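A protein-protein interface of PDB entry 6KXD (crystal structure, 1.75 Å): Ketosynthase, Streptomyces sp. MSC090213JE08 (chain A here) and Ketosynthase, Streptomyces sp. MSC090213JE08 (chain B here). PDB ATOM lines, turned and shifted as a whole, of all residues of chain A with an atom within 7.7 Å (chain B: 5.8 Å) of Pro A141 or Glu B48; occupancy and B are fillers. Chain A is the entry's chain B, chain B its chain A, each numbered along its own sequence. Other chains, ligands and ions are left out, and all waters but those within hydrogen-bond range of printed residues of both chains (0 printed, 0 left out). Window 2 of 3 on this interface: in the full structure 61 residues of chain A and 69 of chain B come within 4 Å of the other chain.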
ATOM      1  N   PHE A 131       8.888  -7.189 -19.406  1.00  0.00           N
ATOM      2  CA  PHE A 131       9.816  -7.424 -18.344  1.00  0.00           C
ATOM      3  C   PHE A 131      10.809  -6.260 -18.308  1.00  0.00           C
ATOM      4  O   PHE A 131      11.075  -5.646 -17.268  1.00  0.00           O
ATOM      5  CB  PHE A 131      10.525  -8.756 -18.536  1.00  0.00           C
ATOM      6  CG  PHE A 131      11.647  -9.079 -17.588  1.00  0.00           C
ATOM      7  CD1 PHE A 131      12.924  -8.575 -17.757  1.00  0.00           C
ATOM      8  CD2 PHE A 131      11.431  -9.948 -16.530  1.00  0.00           C
ATOM      9  CE1 PHE A 131      13.944  -8.908 -16.883  1.00  0.00           C
ATOM     10  CE2 PHE A 131      12.466 -10.311 -15.683  1.00  0.00           C
ATOM     11  CZ  PHE A 131      13.716  -9.786 -15.846  1.00  0.00           C
ATOM     12  N   LEU A 132      11.356  -5.933 -19.471  1.00  0.00           N
ATOM     13  CA  LEU A 132      12.368  -4.868 -19.477  1.00  0.00           C
ATOM     14  C   LEU A 132      11.724  -3.507 -19.206  1.00  0.00           C
ATOM     15  O   LEU A 132      12.345  -2.673 -18.503  1.00  0.00           O
ATOM     16  CB  LEU A 132      13.131  -4.905 -20.797  1.00  0.00           C
ATOM     17  CG  LEU A 132      14.115  -6.064 -20.908  1.00  0.00           C
ATOM     18  CD1 LEU A 132      14.635  -6.176 -22.324  1.00  0.00           C
ATOM     19  CD2 LEU A 132      15.275  -5.916 -19.950  1.00  0.00           C
ATOM     20  N   GLN A 134       9.333  -2.951 -17.239  1.00  0.00           N
ATOM     21  CA  GLN A 134       9.162  -2.920 -15.802  1.00  0.00           C
ATOM     22  C   GLN A 134      10.507  -2.641 -15.124  1.00  0.00           C
ATOM     23  O   GLN A 134      10.599  -1.812 -14.209  1.00  0.00           O
ATOM     24  CB  GLN A 134       8.521  -4.219 -15.304  1.00  0.00           C
ATOM     25  CG  GLN A 134       7.048  -4.352 -15.650  1.00  0.00           C
ATOM     26  CD  GLN A 134       6.607  -5.796 -15.594  1.00  0.00           C
ATOM     27  OE1 GLN A 134       7.366  -6.688 -15.210  1.00  0.00           O
ATOM     28  NE2 GLN A 134       5.387  -6.049 -16.035  1.00  0.00           N
ATOM     29  N   SER A 135      11.554  -3.311 -15.594  1.00  0.00           N
ATOM     30  CA  SER A 135      12.859  -3.164 -15.106  1.00  0.00           C
ATOM     31  C   SER A 135      13.286  -1.693 -15.151  1.00  0.00           C
ATOM     32  O   SER A 135      13.974  -1.250 -14.279  1.00  0.00           O
ATOM     33  CB  SER A 135      13.805  -3.978 -15.918  1.00  0.00           C
ATOM     34  OG  SER A 135      15.127  -3.787 -15.477  1.00  0.00           O
ATOM     35  N   TYR A 136      12.914  -0.992 -16.216  1.00  0.00           N
ATOM     36  CA  TYR A 136      13.383   0.385 -16.419  1.00  0.00           C
ATOM     37  C   TYR A 136      12.554   1.379 -15.596  1.00  0.00           C
ATOM     38  O   TYR A 136      13.092   2.389 -15.164  1.00  0.00           O
ATOM     39  CB  TYR A 136      13.374   0.772 -17.900  1.00  0.00           C
ATOM     40  CG  TYR A 136      14.582   0.270 -18.650  1.00  0.00           C
ATOM     41  CD1 TYR A 136      15.857   0.709 -18.324  1.00  0.00           C
ATOM     42  CD2 TYR A 136      14.464  -0.665 -19.671  1.00  0.00           C
ATOM     43  CE1 TYR A 136      16.985   0.248 -18.990  1.00  0.00           C
ATOM     44  CE2 TYR A 136      15.579  -1.147 -20.330  1.00  0.00           C
ATOM     45  CZ  TYR A 136      16.842  -0.689 -20.003  1.00  0.00           C
ATOM     46  OH  TYR A 136      17.938  -1.150 -20.675  1.00  0.00           O
ATOM     47  N   THR A 137      11.261   1.107 -15.424  1.00  0.00           N
ATOM     48  CA  THR A 137      10.280   2.123 -14.989  1.00  0.00           C
ATOM     49  C   THR A 137       9.765   1.884 -13.555  1.00  0.00           C
ATOM     50  O   THR A 137       9.136   2.759 -12.991  1.00  0.00           O
ATOM     51  CB  THR A 137       9.088   2.166 -15.948  1.00  0.00           C
ATOM     52  OG1 THR A 137       8.439   0.894 -15.898  1.00  0.00           O
ATOM     53  CG2 THR A 137       9.488   2.524 -17.364  1.00  0.00           C
ATOM     54  N   ASN A 138      10.027   0.711 -12.977  1.00  0.00           N
ATOM     55  CA  ASN A 138       9.561   0.375 -11.634  1.00  0.00           C
ATOM     56  C   ASN A 138      10.593   0.861 -10.610  1.00  0.00           C
ATOM     57  O   ASN A 138      11.553   1.511 -10.968  1.00  0.00           O
ATOM     58  CB  ASN A 138       9.242  -1.114 -11.500  1.00  0.00           C
ATOM     59  CG  ASN A 138       7.875  -1.460 -12.046  1.00  0.00           C
ATOM     60  OD1 ASN A 138       7.111  -0.557 -12.385  1.00  0.00           O
ATOM     61  ND2 ASN A 138       7.580  -2.753 -12.152  1.00  0.00           N
ATOM     62  N   ALA A 139      10.361   0.547  -9.333  1.00  0.00           N
ATOM     63  CA  ALA A 139      11.074   1.161  -8.223  1.00  0.00           C
ATOM     64  C   ALA A 139      12.542   0.757  -8.263  1.00  0.00           C
ATOM     65  O   ALA A 139      13.426   1.588  -8.046  1.00  0.00           O
ATOM     66  CB  ALA A 139      10.451   0.760  -6.906  1.00  0.00           C
ATOM     67  N   ARG A 140      12.761  -0.544  -8.455  1.00  0.00           N
ATOM     68  CA  ARG A 140      14.057  -1.086  -8.620  1.00  0.00           C
ATOM     69  C   ARG A 140      14.055  -1.897  -9.916  1.00  0.00           C
ATOM     70  O   ARG A 140      12.985  -2.239 -10.427  1.00  0.00           O
ATOM     71  CB  ARG A 140      14.440  -1.817  -7.336  1.00  0.00           C
ATOM     72  CG  ARG A 140      14.675  -0.838  -6.187  1.00  0.00           C
ATOM     73  CD  ARG A 140      15.206  -1.457  -4.920  1.00  0.00           C
ATOM     74  NE  ARG A 140      16.543  -2.014  -5.044  1.00  0.00           N
ATOM     75  CZ  ARG A 140      16.986  -3.028  -4.314  1.00  0.00           C
ATOM     76  NH1 ARG A 140      16.178  -3.631  -3.459  1.00  0.00           N
ATOM     77  NH2 ARG A 140      18.230  -3.447  -4.438  1.00  0.00           N
ATOM     78  N   PRO A 141      15.234  -2.147 -10.517  1.00  0.00           N
ATOM     79  CA  PRO A 141      15.293  -2.721 -11.869  1.00  0.00           C
ATOM     80  C   PRO A 141      15.041  -4.240 -11.957  1.00  0.00           C
ATOM     81  O   PRO A 141      15.182  -4.834 -13.036  1.00  0.00           O
ATOM     82  CB  PRO A 141      16.725  -2.380 -12.301  1.00  0.00           C
ATOM     83  CG  PRO A 141      17.510  -2.424 -11.019  1.00  0.00           C
ATOM     84  CD  PRO A 141      16.568  -1.845  -9.981  1.00  0.00           C
ATOM     85  N   PHE A 142      14.737  -4.875 -10.825  1.00  0.00           N
ATOM     86  CA  PHE A 142      14.363  -6.284 -10.799  1.00  0.00           C
ATOM     87  C   PHE A 142      12.968  -6.429 -10.200  1.00  0.00           C
ATOM     88  O   PHE A 142      12.571  -7.546  -9.856  1.00  0.00           O
ATOM     89  CB  PHE A 142      15.421  -7.076 -10.046  1.00  0.00           C
ATOM     90  CG  PHE A 142      15.561  -6.723  -8.591  1.00  0.00           C
ATOM     91  CD1 PHE A 142      16.312  -5.625  -8.200  1.00  0.00           C
ATOM     92  CD2 PHE A 142      14.997  -7.526  -7.613  1.00  0.00           C
ATOM     93  CE1 PHE A 142      16.482  -5.328  -6.857  1.00  0.00           C
ATOM     94  CE2 PHE A 142      15.167  -7.228  -6.270  1.00  0.00           C
ATOM     95  CZ  PHE A 142      15.907  -6.127  -5.895  1.00  0.00           C
ATOM     96  N   TYR A 143      12.249  -5.301 -10.135  1.00  0.00           N
ATOM     97  CA  TYR A 143      10.843  -5.222  -9.720  1.00  0.00           C
ATOM     98  C   TYR A 143       9.955  -5.426 -10.953  1.00  0.00           C
ATOM     99  O   TYR A 143       9.312  -4.531 -11.492  1.00  0.00           O
ATOM    100  CB  TYR A 143      10.572  -3.935  -8.935  1.00  0.00           C
ATOM    101  CG  TYR A 143      11.162  -3.946  -7.534  1.00  0.00           C
ATOM    102  CD1 TYR A 143      12.132  -4.883  -7.164  1.00  0.00           C
ATOM    103  CD2 TYR A 143      10.798  -2.992  -6.582  1.00  0.00           C
ATOM    104  CE1 TYR A 143      12.688  -4.913  -5.889  1.00  0.00           C
ATOM    105  CE2 TYR A 143      11.359  -2.996  -5.300  1.00  0.00           C
ATOM    106  CZ  TYR A 143      12.303  -3.959  -4.954  1.00  0.00           C
ATOM    107  OH  TYR A 143      12.886  -4.013  -3.716  1.00  0.00           O
ATOM    108  N   VAL A 144       9.899  -6.697 -11.342  1.00  0.00           N
ATOM    109  CA  VAL A 144       9.179  -7.146 -12.502  1.00  0.00           C
ATOM    110  C   VAL A 144       7.991  -7.995 -12.036  1.00  0.00           C
ATOM    111  O   VAL A 144       7.963  -8.459 -10.862  1.00  0.00           O
ATOM    112  CB  VAL A 144      10.122  -7.969 -13.401  1.00  0.00           C
ATOM    113  CG1 VAL A 144      11.332  -7.162 -13.832  1.00  0.00           C
ATOM    114  CG2 VAL A 144      10.575  -9.249 -12.722  1.00  0.00           C
ATOM    115  N   ASP B  46      23.908  -0.616 -16.935  1.00  0.00           N
ATOM    116  CA  ASP B  46      23.770   0.157 -15.709  1.00  0.00           C
ATOM    117  C   ASP B  46      23.237  -0.782 -14.615  1.00  0.00           C
ATOM    118  O   ASP B  46      22.141  -1.320 -14.749  1.00  0.00           O
ATOM    119  CB  ASP B  46      22.852   1.342 -16.047  1.00  0.00           C
ATOM    120  CG  ASP B  46      22.587   2.354 -14.945  1.00  0.00           C
ATOM    121  OD1 ASP B  46      23.211   2.247 -13.878  1.00  0.00           O
ATOM    122  OD2 ASP B  46      21.745   3.257 -15.184  1.00  0.00           O
ATOM    123  N   THR B  47      24.024  -1.003 -13.554  1.00  0.00           N
ATOM    124  CA  THR B  47      23.653  -1.898 -12.447  1.00  0.00           C
ATOM    125  C   THR B  47      22.999  -1.133 -11.279  1.00  0.00           C
ATOM    126  O   THR B  47      22.575  -1.760 -10.304  1.00  0.00           O
ATOM    127  CB  THR B  47      24.852  -2.718 -11.960  1.00  0.00           C
ATOM    128  OG1 THR B  47      25.866  -1.876 -11.410  1.00  0.00           O
ATOM    129  CG2 THR B  47      25.470  -3.556 -13.054  1.00  0.00           C
ATOM    130  N   GLU B  48      22.884   0.198 -11.393  1.00  0.00           N
ATOM    131  CA  GLU B  48      22.191   1.039 -10.428  1.00  0.00           C
ATOM    132  C   GLU B  48      20.864   0.380 -10.049  1.00  0.00           C
ATOM    133  O   GLU B  48      19.972   0.226 -10.879  1.00  0.00           O
ATOM    134  CB  GLU B  48      21.895   2.425 -11.021  1.00  0.00           C
ATOM    135  CG  GLU B  48      20.946   3.297 -10.196  1.00  0.00           C
ATOM    136  CD  GLU B  48      20.313   4.490 -10.914  1.00  0.00           C
ATOM    137  OE1 GLU B  48      19.315   5.042 -10.392  1.00  0.00           O
ATOM    138  OE2 GLU B  48      20.805   4.874 -11.995  1.00  0.00           O
ATOM    139  N   GLY B  49      20.712   0.055  -8.765  1.00  0.00           N
ATOM    140  CA  GLY B  49      19.397  -0.243  -8.238  1.00  0.00           C
ATOM    141  C   GLY B  49      19.239  -1.723  -7.960  1.00  0.00           C
ATOM    142  O   GLY B  49      18.292  -2.114  -7.320  1.00  0.00           O
ATOM    143  N   PHE B  50      20.168  -2.533  -8.476  1.00  0.00           N
ATOM    144  CA  PHE B  50      20.134  -3.986  -8.319  1.00  0.00           C
ATOM    145  C   PHE B  50      20.721  -4.387  -6.965  1.00  0.00           C
ATOM    146  O   PHE B  50      20.619  -5.565  -6.581  1.00  0.00           O
ATOM    147  CB  PHE B  50      20.936  -4.675  -9.434  1.00  0.00           C
ATOM    148  CG  PHE B  50      20.216  -4.756 -10.750  1.00  0.00           C
ATOM    149  CD1 PHE B  50      19.339  -5.795 -10.992  1.00  0.00           C
ATOM    150  CD2 PHE B  50      20.412  -3.812 -11.750  1.00  0.00           C
ATOM    151  CE1 PHE B  50      18.663  -5.876 -12.198  1.00  0.00           C
ATOM    152  CE2 PHE B  50      19.738  -3.905 -12.958  1.00  0.00           C
ATOM    153  CZ  PHE B  50      18.838  -4.919 -13.167  1.00  0.00           C
ATOM    154  N   GLY B  51      21.386  -3.427  -6.297  1.00  0.00           N
ATOM    155  CA  GLY B  51      22.066  -3.633  -5.024  1.00  0.00           C
ATOM    156  C   GLY B  51      23.288  -4.507  -5.192  1.00  0.00           C
ATOM    157  O   GLY B  51      23.824  -5.012  -4.244  1.00  0.00           O
ATOM    158  N   ARG B 202      20.867  -7.025 -19.051  1.00  0.00           N
ATOM    159  CA  ARG B 202      20.038  -6.615 -17.948  1.00  0.00           C
ATOM    160  C   ARG B 202      18.895  -7.627 -17.752  1.00  0.00           C
ATOM    161  O   ARG B 202      18.580  -7.981 -16.619  1.00  0.00           O
ATOM    162  CB  ARG B 202      19.548  -5.206 -18.225  1.00  0.00           C
ATOM    163  CG  ARG B 202      18.528  -4.686 -17.239  1.00  0.00           C
ATOM    164  CD  ARG B 202      18.032  -3.362 -17.779  1.00  0.00           C
ATOM    165  NE  ARG B 202      17.190  -2.695 -16.807  1.00  0.00           N
ATOM    166  CZ  ARG B 202      17.525  -1.602 -16.141  1.00  0.00           C
ATOM    167  NH1 ARG B 202      18.772  -1.159 -16.150  1.00  0.00           N
ATOM    168  NH2 ARG B 202      16.582  -0.922 -15.523  1.00  0.00           N
ATOM    169  N   ALA B 206      18.429  -9.218 -14.061  1.00  0.00           N
ATOM    170  CA  ALA B 206      17.179  -8.894 -13.384  1.00  0.00           C
ATOM    171  C   ALA B 206      16.322 -10.139 -13.162  1.00  0.00           C
ATOM    172  O   ALA B 206      15.717 -10.299 -12.094  1.00  0.00           O
ATOM    173  CB  ALA B 206      16.424  -7.869 -14.156  1.00  0.00           C
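O of Gly B49 sits at hydrogen-bond distance from NE of Arg A140 (2.9 Å).
The guanidinium group (NE) of Arg B202 lies within hydrogen-bond range of the side-chain hydroxyl (OG) of Ser A135 (2.7 Å).
The side-chain carboxylate (OD1) of Asp B46 sits close to the backbone NH (N) of Glu B48 (3.2 Å).
OG of Ser A135 sits at hydrogen-bond distance from O of Pro A141 (2.7 Å).
The side-chain hydroxyl of Tyr A143 lies within hydrogen-bond range of the guanidinium group of Arg A140 (3.3 Å).
Among the printed residues, pairs that only touch across the chains: Pro A141 with Gly B49 (3.2 Å), Pro A141 with Phe B50 (3.3 Å), Tyr A136 with Arg B202 (3.3 Å), Pro A141 with Ala B206 (3.5 Å), Pro A141 with Arg B202 (3.5 Å), Pro A141 with Glu B48 (3.6 Å), Arg A140 with Gly B51 (3.7 Å), Arg A140 with Phe B50 (3.7 Å), Phe A142 with Gly B49 (3.7 Å), Phe A131 with Ala B206 (3.7 Å) and Phe A142 with Ala B206 (3.8 Å).
Pro A141 touches five residues of chain B.
Of chain A, only Pro A141 comes within 4 Å of Glu B48.
Of the printed residues of chain A, Ala B206 touches Phe A131 (3.7 Å), Pro A141 (3.5 Å) and Phe A142 (3.8 Å).
Printed residues of chain B within 4 Å of Phe A142: Gly B49 and Ala B206.
Of the printed residues of chain B, Tyr A136 touches Arg B202 (3.3 Å).
The nearest residue of chain B that does not touch Pro A141 is Thr B47 (5.2 Å).
The nearest printed residue of chain A that does not touch Phe B50 is Phe A142 (4.1 Å).
Of the 13 printed residues of chain A, 6 touch a printed residue of chain B.
Of the 8 printed residues of chain B, 6 touch a printed residue of chain A.
Printed residues of chain B that touch a printed residue of chain A: Glu B48, Gly B49, Phe B50, Gly B51, Arg B202 and Ala B206.
Hydrophobic or aromatic side chains of chain B within 4 Å of the printed part of chain A: Phe B50 and Ala B206.
Among the printed residues, 13 pairs touch across the chains.
Among the printed residues, no Asp or Glu carboxylate lies within 4 Å of a Lys or Arg side-chain nitrogen of the other chain.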
